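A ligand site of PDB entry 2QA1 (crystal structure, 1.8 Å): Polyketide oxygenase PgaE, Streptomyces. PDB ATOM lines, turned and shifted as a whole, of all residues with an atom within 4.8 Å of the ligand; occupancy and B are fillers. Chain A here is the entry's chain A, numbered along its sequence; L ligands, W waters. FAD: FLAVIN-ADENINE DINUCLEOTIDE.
OE2 of Glu 41 sits at hydrogen-bond distance from O2B of the ligand (2.5 Å). An oxygen (O2') of the ligand is in hydrogen-bond range of the side-chain amide oxygen of Gln 105 (2.7 Å). O2A of the ligand lies within salt-bridge range of NH2 of Arg 51, at 3.2 Å. The backbone NH (N) of Asn 298 sits at hydrogen-bond distance from an oxygen (O2) of the ligand (3.0 Å). An oxygen (O2) of the ligand sits at hydrogen-bond distance from the side-chain amide nitrogen (ND2) of Asn 298, at 2.8 Å. An oxygen (O1P) of the ligand is in hydrogen-bond range of the backbone NH of Asp 284, at 2.9 Å. The side-chain carboxylate (OD1) of Asp 284 sits at hydrogen-bond distance from an oxygen (O3') of the ligand (2.8 Å). N of Met 297 lies within hydrogen-bond range of N1 of the ligand (2.9 Å). N of Val 129 sits at hydrogen-bond distance from N1A of the ligand. O of Val 129 is in hydrogen-bond range of N6A of the ligand (2.9 Å). N of Ala 22 lies within hydrogen-bond range of O2P of the ligand, at 3.0 Å. N1 of the ligand sits at hydrogen-bond distance from N of Gly 296, 3.4 Å away. A nitrogen (N3A) of the ligand is in hydrogen-bond range of the backbone NH of Arg 42, at 3.1 Å. An oxygen (O2B) of the ligand sits at hydrogen-bond distance from the guanidinium group (NE) of Arg 42 (3.1 Å). N6A of the ligand lies within hydrogen-bond range of OG of Ser 166, 3.4 Å away.
The backbone NH (N) of Gln 105 lies within hydrogen-bond range of the backbone carbonyl oxygen (O) of Gly 52, 2.8 Å away. The side-chain carboxylate of Glu 109 lies within hydrogen-bond range of the side-chain amide nitrogen of Gln 105. The side-chain amide nitrogen (ND2) of Asn 298 lies within hydrogen-bond range of the backbone carbonyl oxygen (O) of Gly 294 (2.9 Å). The backbone carbonyl oxygen (O) of Gly 296 sits at hydrogen-bond distance from the side-chain hydroxyl (OG) of Ser 300 (2.9 Å). The backbone carbonyl oxygen (O) of Leu 40 lies within hydrogen-bond range of the backbone NH (N) of Gly 18 (2.7 Å). The side-chain carboxylate (OD2) of Asp 161 sits at hydrogen-bond distance from the backbone NH (N) of Ser 166 (3.0 Å). O of Val 17 lies within hydrogen-bond range of N of Cys 160 (2.8 Å). The backbone carbonyl oxygen (O) of Gly 162 lies close to the backbone NH (N) of Ser 285 (3.5 Å).
O2P of the ligand lies close to N of Pro 21 (3.3 Å). The backbone carbonyl oxygen (O) of Leu 40 lies close to a nitrogen (N3A) of the ligand, at 3.5 Å. Merely in contact with the ligand: Val 17, Gly 18, Gly 20, Leu 43, Gly 52, Leu 53, His 127, Glu 128, Cys 160, Asp 161, Gly 162, Leu 186, Phe 264, Gly 283, Pro 291, Gly 294, Gln 295 and Ser 300. Of the 36 residues printed, 31 come within 4 Å of the ligand. The nearest printed residue that does not touch the ligand is Ala 19 (4.1 Å).
Water W2 bridges O1A of the ligand and OE2 of Glu 109. Water W4 lies within hydrogen-bond range of O2P of the ligand (2.7 Å), O of Cys 160 (2.7 Å), N of Gly 20 (2.8 Å) and N of Gly 23 (3.0 Å). Water W11 lies within hydrogen-bond range of an oxygen (O2A) of the ligand (2.7 Å) and the side-chain carboxylate of Asp 284 (2.7 Å). Water W7 lies within hydrogen-bond range of O4 of the ligand (2.7 Å) and O of Leu 53 (3.1 Å). Water W8 bridges the side-chain hydroxyl (OG) of Ser 166 (2.7 Å) and a nitrogen (N7A) of the ligand (2.8 Å). Water W9 lies within hydrogen-bond range of N3 of the ligand (2.8 Å) and ND2 of Asn 298 (2.9 Å).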
ATOM      1  N   VAL A  17      12.098  -6.884  34.928  1.00  0.00           N
ATOM      2  CA  VAL A  17      12.182  -5.563  34.303  1.00  0.00           C
ATOM      3  C   VAL A  17      11.067  -5.423  33.259  1.00  0.00           C
ATOM      4  O   VAL A  17      11.047  -6.155  32.272  1.00  0.00           O
ATOM      5  CB  VAL A  17      13.576  -5.335  33.625  1.00  0.00           C
ATOM      6  CG1 VAL A  17      13.718  -3.894  33.131  1.00  0.00           C
ATOM      7  CG2 VAL A  17      14.708  -5.650  34.595  1.00  0.00           C
ATOM      8  N   GLY A  18      10.152  -4.486  33.485  1.00  0.00           N
ATOM      9  CA  GLY A  18       9.085  -4.236  32.525  1.00  0.00           C
ATOM     10  C   GLY A  18       7.751  -4.757  33.017  1.00  0.00           C
ATOM     11  O   GLY A  18       7.649  -5.895  33.485  1.00  0.00           O
ATOM     12  N   ALA A  19       6.727  -3.921  32.922  1.00  0.00           N
ATOM     13  CA  ALA A  19       5.379  -4.281  33.344  1.00  0.00           C
ATOM     14  C   ALA A  19       4.422  -4.229  32.138  1.00  0.00           C
ATOM     15  O   ALA A  19       3.295  -3.753  32.251  1.00  0.00           O
ATOM     16  CB  ALA A  19       4.907  -3.362  34.487  1.00  0.00           C
ATOM     17  N   GLY A  20       4.888  -4.740  30.999  1.00  0.00           N
ATOM     18  CA  GLY A  20       4.000  -5.124  29.905  1.00  0.00           C
ATOM     19  C   GLY A  20       3.326  -6.461  30.204  1.00  0.00           C
ATOM     20  O   GLY A  20       3.387  -6.960  31.344  1.00  0.00           O
ATOM     21  N   PRO A  21       2.637  -7.044  29.211  1.00  0.00           N
ATOM     22  CA  PRO A  21       1.940  -8.318  29.430  1.00  0.00           C
ATOM     23  C   PRO A  21       2.848  -9.453  29.923  1.00  0.00           C
ATOM     24  O   PRO A  21       2.442 -10.217  30.801  1.00  0.00           O
ATOM     25  CB  PRO A  21       1.351  -8.663  28.053  1.00  0.00           C
ATOM     26  CG  PRO A  21       1.854  -7.685  27.112  1.00  0.00           C
ATOM     27  CD  PRO A  21       2.466  -6.537  27.844  1.00  0.00           C
ATOM     28  N   ALA A  22       4.072  -9.535  29.397  1.00  0.00           N
ATOM     29  CA  ALA A  22       4.993 -10.590  29.819  1.00  0.00           C
ATOM     30  C   ALA A  22       5.370 -10.418  31.298  1.00  0.00           C
ATOM     31  O   ALA A  22       5.260 -11.361  32.093  1.00  0.00           O
ATOM     32  CB  ALA A  22       6.260 -10.603  28.925  1.00  0.00           C
ATOM     33  N   GLY A  23       5.793  -9.219  31.665  1.00  0.00           N
ATOM     34  CA  GLY A  23       6.220  -8.945  33.029  1.00  0.00           C
ATOM     35  C   GLY A  23       5.123  -9.105  34.045  1.00  0.00           C
ATOM     36  O   GLY A  23       5.341  -9.636  35.145  1.00  0.00           O
ATOM     37  N   LEU A  40      10.262  -3.708  38.022  1.00  0.00           N
ATOM     38  CA  LEU A  40      10.758  -2.353  37.790  1.00  0.00           C
ATOM     39  C   LEU A  40      10.227  -1.940  36.428  1.00  0.00           C
ATOM     40  O   LEU A  40      10.533  -2.568  35.399  1.00  0.00           O
ATOM     41  CB  LEU A  40      12.289  -2.292  37.835  1.00  0.00           C
ATOM     42  CG  LEU A  40      12.931  -2.801  39.139  1.00  0.00           C
ATOM     43  CD1 LEU A  40      14.441  -2.853  39.003  1.00  0.00           C
ATOM     44  CD2 LEU A  40      12.513  -1.951  40.336  1.00  0.00           C
ATOM     45  N   GLU A  41       9.379  -0.915  36.423  1.00  0.00           N
ATOM     46  CA  GLU A  41       8.829  -0.386  35.177  1.00  0.00           C
ATOM     47  C   GLU A  41       9.124   1.107  35.056  1.00  0.00           C
ATOM     48  O   GLU A  41       8.831   1.872  35.960  1.00  0.00           O
ATOM     49  CB  GLU A  41       7.313  -0.669  35.131  1.00  0.00           C
ATOM     50  CG  GLU A  41       6.548   0.108  34.072  1.00  0.00           C
ATOM     51  CD  GLU A  41       6.977  -0.215  32.643  1.00  0.00           C
ATOM     52  OE1 GLU A  41       6.984  -1.411  32.253  1.00  0.00           O
ATOM     53  OE2 GLU A  41       7.294   0.737  31.915  1.00  0.00           O
ATOM     54  N   ARG A  42       9.716   1.504  33.917  1.00  0.00           N
ATOM     55  CA  ARG A  42      10.160   2.901  33.740  1.00  0.00           C
ATOM     56  C   ARG A  42       8.980   3.878  33.672  1.00  0.00           C
ATOM     57  O   ARG A  42       9.066   4.982  34.196  1.00  0.00           O
ATOM     58  CB  ARG A  42      11.056   3.045  32.501  1.00  0.00           C
ATOM     59  CG  ARG A  42      10.403   2.673  31.176  1.00  0.00           C
ATOM     60  CD  ARG A  42      11.370   2.825  29.992  1.00  0.00           C
ATOM     61  NE  ARG A  42      10.763   2.260  28.778  1.00  0.00           N
ATOM     62  CZ  ARG A  42      11.391   2.085  27.620  1.00  0.00           C
ATOM     63  NH1 ARG A  42      12.668   2.416  27.480  1.00  0.00           N
ATOM     64  NH2 ARG A  42      10.729   1.561  26.598  1.00  0.00           N
ATOM     65  N   LEU A  43       7.880   3.451  33.051  1.00  0.00           N
ATOM     66  CA  LEU A  43       6.698   4.298  32.895  1.00  0.00           C
ATOM     67  C   LEU A  43       5.944   4.470  34.197  1.00  0.00           C
ATOM     68  O   LEU A  43       5.722   3.498  34.908  1.00  0.00           O
ATOM     69  CB  LEU A  43       5.735   3.697  31.861  1.00  0.00           C
ATOM     70  CG  LEU A  43       6.218   3.748  30.419  1.00  0.00           C
ATOM     71  CD1 LEU A  43       5.445   2.694  29.610  1.00  0.00           C
ATOM     72  CD2 LEU A  43       6.048   5.153  29.865  1.00  0.00           C
ATOM     73  N   ARG A  51      -2.117  -1.529  20.970  1.00  0.00           N
ATOM     74  CA  ARG A  51      -1.784  -1.874  19.619  1.00  0.00           C
ATOM     75  C   ARG A  51      -2.585  -3.128  19.294  1.00  0.00           C
ATOM     76  O   ARG A  51      -3.377  -3.133  18.354  1.00  0.00           O
ATOM     77  CB  ARG A  51      -0.284  -2.077  19.463  1.00  0.00           C
ATOM     78  CG  ARG A  51       0.428  -2.599  20.681  1.00  0.00           C
ATOM     79  CD  ARG A  51       1.835  -2.008  20.784  1.00  0.00           C
ATOM     80  NE  ARG A  51       2.665  -2.845  21.653  1.00  0.00           N
ATOM     81  CZ  ARG A  51       3.803  -2.463  22.222  1.00  0.00           C
ATOM     82  NH1 ARG A  51       4.284  -1.239  22.050  1.00  0.00           N
ATOM     83  NH2 ARG A  51       4.443  -3.331  22.993  1.00  0.00           N
ATOM     84  N   GLY A  52      -2.446  -4.172  20.107  1.00  0.00           N
ATOM     85  CA  GLY A  52      -3.237  -5.394  19.930  1.00  0.00           C
ATOM     86  C   GLY A  52      -4.712  -5.307  20.344  1.00  0.00           C
ATOM     87  O   GLY A  52      -5.072  -4.549  21.243  1.00  0.00           O
ATOM     88  N   LEU A  53      -5.540  -6.070  19.646  1.00  0.00           N
ATOM     89  CA  LEU A  53      -6.958  -6.240  19.973  1.00  0.00           C
ATOM     90  C   LEU A  53      -7.296  -7.706  20.088  1.00  0.00           C
ATOM     91  O   LEU A  53      -7.011  -8.501  19.191  1.00  0.00           O
ATOM     92  CB  LEU A  53      -7.834  -5.651  18.881  1.00  0.00           C
ATOM     93  CG  LEU A  53      -7.819  -4.144  18.653  1.00  0.00           C
ATOM     94  CD1 LEU A  53      -8.561  -3.864  17.364  1.00  0.00           C
ATOM     95  CD2 LEU A  53      -8.423  -3.398  19.838  1.00  0.00           C
ATOM     96  N   GLN A 105      -5.294  -4.356  24.071  1.00  0.00           N
ATOM     97  CA  GLN A 105      -4.150  -4.807  24.856  1.00  0.00           C
ATOM     98  C   GLN A 105      -4.047  -4.069  26.200  1.00  0.00           C
ATOM     99  O   GLN A 105      -3.684  -4.680  27.211  1.00  0.00           O
ATOM    100  CB  GLN A 105      -2.840  -4.685  24.072  1.00  0.00           C
ATOM    101  CG  GLN A 105      -1.598  -4.986  24.900  1.00  0.00           C
ATOM    102  CD  GLN A 105      -0.327  -5.157  24.068  1.00  0.00           C
ATOM    103  OE1 GLN A 105      -0.375  -5.397  22.853  1.00  0.00           O
ATOM    104  NE2 GLN A 105       0.813  -5.044  24.732  1.00  0.00           N
ATOM    105  N   GLU A 109      -3.624  -5.787  29.848  1.00  0.00           N
ATOM    106  CA  GLU A 109      -2.510  -5.386  30.711  1.00  0.00           C
ATOM    107  C   GLU A 109      -3.004  -4.925  32.085  1.00  0.00           C
ATOM    108  O   GLU A 109      -2.415  -5.269  33.108  1.00  0.00           O
ATOM    109  CB  GLU A 109      -1.690  -4.271  30.058  1.00  0.00           C
ATOM    110  CG  GLU A 109      -0.868  -4.721  28.849  1.00  0.00           C
ATOM    111  CD  GLU A 109      -0.020  -3.590  28.259  1.00  0.00           C
ATOM    112  OE1 GLU A 109       0.023  -2.501  28.837  1.00  0.00           O
ATOM    113  OE2 GLU A 109       0.615  -3.804  27.222  1.00  0.00           O
ATOM    114  N   HIS A 127      10.547   3.494  37.710  1.00  0.00           N
ATOM    115  CA  HIS A 127      11.857   2.935  38.000  1.00  0.00           C
ATOM    116  C   HIS A 127      12.419   2.349  36.729  1.00  0.00           C
ATOM    117  O   HIS A 127      11.916   1.331  36.218  1.00  0.00           O
ATOM    118  CB  HIS A 127      11.733   1.822  39.041  1.00  0.00           C
ATOM    119  CG  HIS A 127      11.477   2.325  40.417  1.00  0.00           C
ATOM    120  ND1 HIS A 127      10.302   2.946  40.784  1.00  0.00           N
ATOM    121  CD2 HIS A 127      12.256   2.310  41.530  1.00  0.00           C
ATOM    122  CE1 HIS A 127      10.358   3.278  42.062  1.00  0.00           C
ATOM    123  NE2 HIS A 127      11.529   2.901  42.534  1.00  0.00           N
ATOM    124  N   GLU A 128      13.457   3.008  36.233  1.00  0.00           N
ATOM    125  CA  GLU A 128      14.134   2.579  35.020  1.00  0.00           C
ATOM    126  C   GLU A 128      15.435   1.860  35.375  1.00  0.00           C
ATOM    127  O   GLU A 128      16.299   2.431  36.062  1.00  0.00           O
ATOM    128  CB  GLU A 128      14.432   3.767  34.103  1.00  0.00           C
ATOM    129  CG  GLU A 128      14.987   3.356  32.737  1.00  0.00           C
ATOM    130  CD  GLU A 128      15.076   4.516  31.767  1.00  0.00           C
ATOM    131  OE1 GLU A 128      15.500   5.607  32.187  1.00  0.00           O
ATOM    132  OE2 GLU A 128      14.748   4.311  30.576  1.00  0.00           O
ATOM    133  N   VAL A 129      15.564   0.619  34.915  1.00  0.00           N
ATOM    134  CA  VAL A 129      16.843  -0.078  34.968  1.00  0.00           C
ATOM    135  C   VAL A 129      17.812   0.476  33.934  1.00  0.00           C
ATOM    136  O   VAL A 129      17.612   0.332  32.734  1.00  0.00           O
ATOM    137  CB  VAL A 129      16.675  -1.593  34.732  1.00  0.00           C
ATOM    138  CG1 VAL A 129      18.030  -2.271  34.660  1.00  0.00           C
ATOM    139  CG2 VAL A 129      15.813  -2.211  35.828  1.00  0.00           C
ATOM    140  N   CYS A 160      11.762  -8.505  30.848  1.00  0.00           N
ATOM    141  CA  CYS A 160      10.486  -8.422  30.123  1.00  0.00           C
ATOM    142  C   CYS A 160      10.306  -6.999  29.599  1.00  0.00           C
ATOM    143  O   CYS A 160       9.209  -6.420  29.633  1.00  0.00           O
ATOM    144  CB  CYS A 160       9.297  -8.802  31.015  1.00  0.00           C
ATOM    145  SG  CYS A 160       9.430 -10.419  31.754  1.00  0.00           S
ATOM    146  N   ASP A 161      11.402  -6.448  29.090  1.00  0.00           N
ATOM    147  CA  ASP A 161      11.486  -5.028  28.821  1.00  0.00           C
ATOM    148  C   ASP A 161      11.361  -4.652  27.345  1.00  0.00           C
ATOM    149  O   ASP A 161      11.812  -3.582  26.929  1.00  0.00           O
ATOM    150  CB  ASP A 161      12.751  -4.424  29.475  1.00  0.00           C
ATOM    151  CG  ASP A 161      14.032  -5.156  29.107  1.00  0.00           C
ATOM    152  OD1 ASP A 161      13.989  -6.358  28.750  1.00  0.00           O
ATOM    153  OD2 ASP A 161      15.108  -4.533  29.235  1.00  0.00           O
ATOM    154  N   GLY A 162      10.729  -5.527  26.564  1.00  0.00           N
ATOM    155  CA  GLY A 162      10.311  -5.179  25.200  1.00  0.00           C
ATOM    156  C   GLY A 162      11.347  -5.341  24.115  1.00  0.00           C
ATOM    157  O   GLY A 162      12.487  -5.736  24.369  1.00  0.00           O
ATOM    158  N   SER A 166      16.920  -3.328  27.197  1.00  0.00           N
ATOM    159  CA  SER A 166      18.197  -2.895  27.819  1.00  0.00           C
ATOM    160  C   SER A 166      18.926  -4.115  28.369  1.00  0.00           C
ATOM    161  O   SER A 166      20.161  -4.186  28.328  1.00  0.00           O
ATOM    162  CB  SER A 166      17.956  -1.949  29.020  1.00  0.00           C
ATOM    163  OG  SER A 166      17.080  -0.863  28.738  1.00  0.00           O
ATOM    164  N   LEU A 186      -0.189   2.723  11.594  1.00  0.00           N
ATOM    165  CA  LEU A 186      -1.544   2.554  12.084  1.00  0.00           C
ATOM    166  C   LEU A 186      -2.038   3.853  12.687  1.00  0.00           C
ATOM    167  O   LEU A 186      -1.252   4.668  13.165  1.00  0.00           O
ATOM    168  CB  LEU A 186      -1.670   1.391  13.083  1.00  0.00           C
ATOM    169  CG  LEU A 186      -1.043   1.511  14.465  1.00  0.00           C
ATOM    170  CD1 LEU A 186      -1.889   0.768  15.488  1.00  0.00           C
ATOM    171  CD2 LEU A 186       0.366   0.989  14.444  1.00  0.00           C
ATOM    172  N   PHE A 264       5.474   1.150  12.675  1.00  0.00           N
ATOM    173  CA  PHE A 264       6.105  -0.135  13.029  1.00  0.00           C
ATOM    174  C   PHE A 264       6.813  -0.763  11.808  1.00  0.00           C
ATOM    175  O   PHE A 264       6.583  -0.350  10.671  1.00  0.00           O
ATOM    176  CB  PHE A 264       5.091  -1.108  13.677  1.00  0.00           C
ATOM    177  CG  PHE A 264       3.944  -1.484  12.785  1.00  0.00           C
ATOM    178  CD1 PHE A 264       4.024  -2.614  11.969  1.00  0.00           C
ATOM    179  CD2 PHE A 264       2.786  -0.722  12.755  1.00  0.00           C
ATOM    180  CE1 PHE A 264       2.967  -2.971  11.126  1.00  0.00           C
ATOM    181  CE2 PHE A 264       1.723  -1.052  11.908  1.00  0.00           C
ATOM    182  CZ  PHE A 264       1.811  -2.188  11.091  1.00  0.00           C
ATOM    183  N   ALA A 282      11.925 -12.907  28.523  1.00  0.00           N
ATOM    184  CA  ALA A 282      10.566 -13.331  28.168  1.00  0.00           C
ATOM    185  C   ALA A 282       9.889 -12.201  27.385  1.00  0.00           C
ATOM    186  O   ALA A 282      10.050 -11.022  27.730  1.00  0.00           O
ATOM    187  CB  ALA A 282       9.756 -13.651  29.423  1.00  0.00           C
ATOM    188  N   GLY A 283       9.150 -12.554  26.345  1.00  0.00           N
ATOM    189  CA  GLY A 283       8.396 -11.569  25.576  1.00  0.00           C
ATOM    190  C   GLY A 283       9.175 -11.008  24.406  1.00  0.00           C
ATOM    191  O   GLY A 283      10.084 -11.674  23.867  1.00  0.00           O
ATOM    192  N   ASP A 284       8.830  -9.782  24.010  1.00  0.00           N
ATOM    193  CA  ASP A 284       9.462  -9.133  22.844  1.00  0.00           C
ATOM    194  C   ASP A 284      10.980  -9.019  23.017  1.00  0.00           C
ATOM    195  O   ASP A 284      11.710  -8.895  22.016  1.00  0.00           O
ATOM    196  CB  ASP A 284       8.893  -7.726  22.638  1.00  0.00           C
ATOM    197  CG  ASP A 284       7.601  -7.708  21.836  1.00  0.00           C
ATOM    198  OD1 ASP A 284       7.025  -8.765  21.506  1.00  0.00           O
ATOM    199  OD2 ASP A 284       7.151  -6.561  21.583  1.00  0.00           O
ATOM    200  N   SER A 285      11.458  -9.044  24.272  1.00  0.00           N
ATOM    201  CA  SER A 285      12.909  -8.910  24.519  1.00  0.00           C
ATOM    202  C   SER A 285      13.646 -10.090  23.901  1.00  0.00           C
ATOM    203  O   SER A 285      14.820  -9.982  23.535  1.00  0.00           O
ATOM    204  CB  SER A 285      13.214  -8.824  26.009  1.00  0.00           C
ATOM    205  OG  SER A 285      12.737  -9.962  26.685  1.00  0.00           O
ATOM    206  N   PRO A 291       4.149  -7.463  13.341  1.00  0.00           N
ATOM    207  CA  PRO A 291       2.932  -7.845  14.062  1.00  0.00           C
ATOM    208  C   PRO A 291       1.836  -8.186  13.047  1.00  0.00           C
ATOM    209  O   PRO A 291       0.923  -7.381  12.787  1.00  0.00           O
ATOM    210  CB  PRO A 291       2.607  -6.613  14.912  1.00  0.00           C
ATOM    211  CG  PRO A 291       3.249  -5.467  14.219  1.00  0.00           C
ATOM    212  CD  PRO A 291       4.289  -6.000  13.228  1.00  0.00           C
ATOM    213  N   GLY A 294      -1.561 -11.514  14.929  1.00  0.00           N
ATOM    214  CA  GLY A 294      -1.940 -11.345  16.336  1.00  0.00           C
ATOM    215  C   GLY A 294      -1.224 -12.330  17.249  1.00  0.00           C
ATOM    216  O   GLY A 294      -1.884 -13.089  17.974  1.00  0.00           O
ATOM    217  N   GLN A 295       0.111 -12.313  17.221  1.00  0.00           N
ATOM    218  CA  GLN A 295       0.928 -13.324  17.929  1.00  0.00           C
ATOM    219  C   GLN A 295       1.808 -12.797  19.059  1.00  0.00           C
ATOM    220  O   GLN A 295       2.115 -13.529  19.971  1.00  0.00           O
ATOM    221  CB  GLN A 295       1.825 -14.075  16.940  1.00  0.00           C
ATOM    222  CG  GLN A 295       1.063 -14.894  15.884  1.00  0.00           C
ATOM    223  CD  GLN A 295       0.269 -16.038  16.506  1.00  0.00           C
ATOM    224  OE1 GLN A 295       0.824 -16.898  17.211  1.00  0.00           O
ATOM    225  NE2 GLN A 295      -1.020 -16.062  16.243  1.00  0.00           N
ATOM    226  N   GLY A 296       2.246 -11.545  18.995  1.00  0.00           N
ATOM    227  CA  GLY A 296       3.305 -11.068  19.897  1.00  0.00           C
ATOM    228  C   GLY A 296       2.903 -11.061  21.372  1.00  0.00           C
ATOM    229  O   GLY A 296       3.563 -11.703  22.219  1.00  0.00           O
ATOM    230  N   MET A 297       1.847 -10.335  21.692  1.00  0.00           N
ATOM    231  CA  MET A 297       1.372 -10.319  23.088  1.00  0.00           C
ATOM    232  C   MET A 297       1.064 -11.731  23.561  1.00  0.00           C
ATOM    233  O   MET A 297       1.432 -12.120  24.673  1.00  0.00           O
ATOM    234  CB  MET A 297       0.133  -9.438  23.281  1.00  0.00           C
ATOM    235  CG  MET A 297      -0.438  -9.476  24.730  1.00  0.00           C
ATOM    236  SD  MET A 297      -2.039  -8.664  24.851  1.00  0.00           S
ATOM    237  CE  MET A 297      -3.063 -10.032  24.275  1.00  0.00           C
ATOM    238  N   ASN A 298       0.380 -12.500  22.728  1.00  0.00           N
ATOM    239  CA  ASN A 298       0.004 -13.859  23.112  1.00  0.00           C
ATOM    240  C   ASN A 298       1.204 -14.734  23.437  1.00  0.00           C
ATOM    241  O   ASN A 298       1.204 -15.425  24.450  1.00  0.00           O
ATOM    242  CB  ASN A 298      -0.839 -14.491  22.005  1.00  0.00           C
ATOM    243  CG  ASN A 298      -2.198 -13.832  21.905  1.00  0.00           C
ATOM    244  OD1 ASN A 298      -3.009 -13.957  22.819  1.00  0.00           O
ATOM    245  ND2 ASN A 298      -2.428 -13.095  20.829  1.00  0.00           N
ATOM    246  N   SER A 300       4.153 -13.679  24.296  1.00  0.00           N
ATOM    247  CA  SER A 300       4.880 -13.075  25.423  1.00  0.00           C
ATOM    248  C   SER A 300       4.245 -13.451  26.755  1.00  0.00           C
ATOM    249  O   SER A 300       4.948 -13.834  27.708  1.00  0.00           O
ATOM    250  CB  SER A 300       4.936 -11.551  25.255  1.00  0.00           C
ATOM    251  OG  SER A 300       5.686 -11.222  24.084  1.00  0.00           O
HETATM  252  PA  FAD L   1       6.151  -4.593  26.120  1.00  0.00           P
HETATM  253  O1A FAD L   1       4.650  -4.731  26.052  1.00  0.00           O
HETATM  254  O2A FAD L   1       6.769  -3.704  25.108  1.00  0.00           O
HETATM  255  O5B FAD L   1       6.543  -4.178  27.641  1.00  0.00           O
HETATM  256  C5B FAD L   1       7.874  -3.708  27.858  1.00  0.00           C
HETATM  257  C4B FAD L   1       7.835  -2.831  29.111  1.00  0.00           C
HETATM  258  O4B FAD L   1       9.134  -2.685  29.640  1.00  0.00           O
HETATM  259  C3B FAD L   1       7.355  -1.436  28.754  1.00  0.00           C
HETATM  260  O3B FAD L   1       6.272  -1.119  29.578  1.00  0.00           O
HETATM  261  C2B FAD L   1       8.561  -0.517  28.972  1.00  0.00           C
HETATM  262  O2B FAD L   1       8.176   0.713  29.554  1.00  0.00           O
HETATM  263  C1B FAD L   1       9.353  -1.335  29.970  1.00  0.00           C
HETATM  264  N9A FAD L   1      10.807  -1.061  29.938  1.00  0.00           N
HETATM  265  C8A FAD L   1      11.694  -1.037  28.881  1.00  0.00           C
HETATM  266  N7A FAD L   1      12.942  -0.772  29.397  1.00  0.00           N
HETATM  267  C5A FAD L   1      12.841  -0.656  30.763  1.00  0.00           C
HETATM  268  C6A FAD L   1      13.773  -0.395  31.809  1.00  0.00           C
HETATM  269  N6A FAD L   1      15.075  -0.230  31.456  1.00  0.00           N
HETATM  270  N1A FAD L   1      13.314  -0.348  33.143  1.00  0.00           N
HETATM  271  C2A FAD L   1      11.966  -0.540  33.469  1.00  0.00           C
HETATM  272  N3A FAD L   1      11.055  -0.809  32.441  1.00  0.00           N
HETATM  273  C4A FAD L   1      11.494  -0.850  31.121  1.00  0.00           C
HETATM  274  N1  FAD L   1       0.197  -8.977  19.785  1.00  0.00           N
HETATM  275  C2  FAD L   1      -0.855  -9.847  19.826  1.00  0.00           C
HETATM  276  O2  FAD L   1      -0.758 -10.866  20.517  1.00  0.00           O
HETATM  277  N3  FAD L   1      -2.003  -9.583  19.110  1.00  0.00           N
HETATM  278  C4  FAD L   1      -2.090  -8.435  18.338  1.00  0.00           C
HETATM  279  O4  FAD L   1      -3.123  -8.192  17.715  1.00  0.00           O
HETATM  280  C4X FAD L   1      -1.014  -7.547  18.289  1.00  0.00           C
HETATM  281  N5  FAD L   1      -1.077  -6.401  17.522  1.00  0.00           N
HETATM  282  C5X FAD L   1      -0.004  -5.519  17.485  1.00  0.00           C
HETATM  283  C6  FAD L   1      -0.106  -4.371  16.686  1.00  0.00           C
HETATM  284  C7  FAD L   1       0.955  -3.468  16.616  1.00  0.00           C
HETATM  285  C7M FAD L   1       0.830  -2.286  15.689  1.00  0.00           C
HETATM  286  C8  FAD L   1       2.115  -3.718  17.358  1.00  0.00           C
HETATM  287  C8M FAD L   1       3.289  -2.780  17.318  1.00  0.00           C
HETATM  288  C9  FAD L   1       2.209  -4.876  18.150  1.00  0.00           C
HETATM  289  C9A FAD L   1       1.146  -5.781  18.211  1.00  0.00           C
HETATM  290  N10 FAD L   1       1.221  -6.949  19.010  1.00  0.00           N
HETATM  291  C10 FAD L   1       0.139  -7.823  19.016  1.00  0.00           C
HETATM  292  C1' FAD L   1       2.452  -7.275  19.782  1.00  0.00           C
HETATM  293  C2' FAD L   1       2.360  -6.883  21.269  1.00  0.00           C
HETATM  294  O2' FAD L   1       1.910  -5.544  21.458  1.00  0.00           O
HETATM  295  C3' FAD L   1       3.731  -7.099  21.906  1.00  0.00           C
HETATM  296  O3' FAD L   1       4.232  -8.353  21.448  1.00  0.00           O
HETATM  297  C4' FAD L   1       3.677  -7.074  23.425  1.00  0.00           C
HETATM  298  O4' FAD L   1       3.450  -5.744  23.880  1.00  0.00           O
HETATM  299  C5' FAD L   1       4.982  -7.587  24.020  1.00  0.00           C
HETATM  300  O5' FAD L   1       4.854  -7.585  25.436  1.00  0.00           O
HETATM  301  P   FAD L   1       6.142  -7.451  26.376  1.00  0.00           P
HETATM  302  O1P FAD L   1       7.137  -8.541  26.048  1.00  0.00           O
HETATM  303  O2P FAD L   1       5.624  -7.585  27.800  1.00  0.00           O
HETATM  304  O3P FAD L   1       6.841  -6.037  26.024  1.00  0.00           O
HETATM  305  O   HOH W   1       7.681  -1.311  24.911  1.00  0.00           O
HETATM  306  O   HOH W   2       3.083  -2.724  26.784  1.00  0.00           O
HETATM  307  O   HOH W   3       1.783  -9.618  16.661  1.00  0.00           O
HETATM  308  O   HOH W   4       6.590  -6.818  30.147  1.00  0.00           O
HETATM  309  O   HOH W   5      -2.833  -6.344  15.355  1.00  0.00           O
HETATM  310  O   HOH W   6       9.783  -8.435  26.734  1.00  0.00           O
HETATM  311  O   HOH W   7      -5.357  -9.458  16.771  1.00  0.00           O
HETATM  312  O   HOH W   8      14.816  -1.450  27.416  1.00  0.00           O
HETATM  313  O   HOH W   9      -4.262 -11.127  19.812  1.00  0.00           O
HETATM  314  O   HOH W  10       4.387  -0.596  27.815  1.00  0.00           O
HETATM  315  O   HOH W  11       8.066  -4.294  22.799  1.00  0.00           O
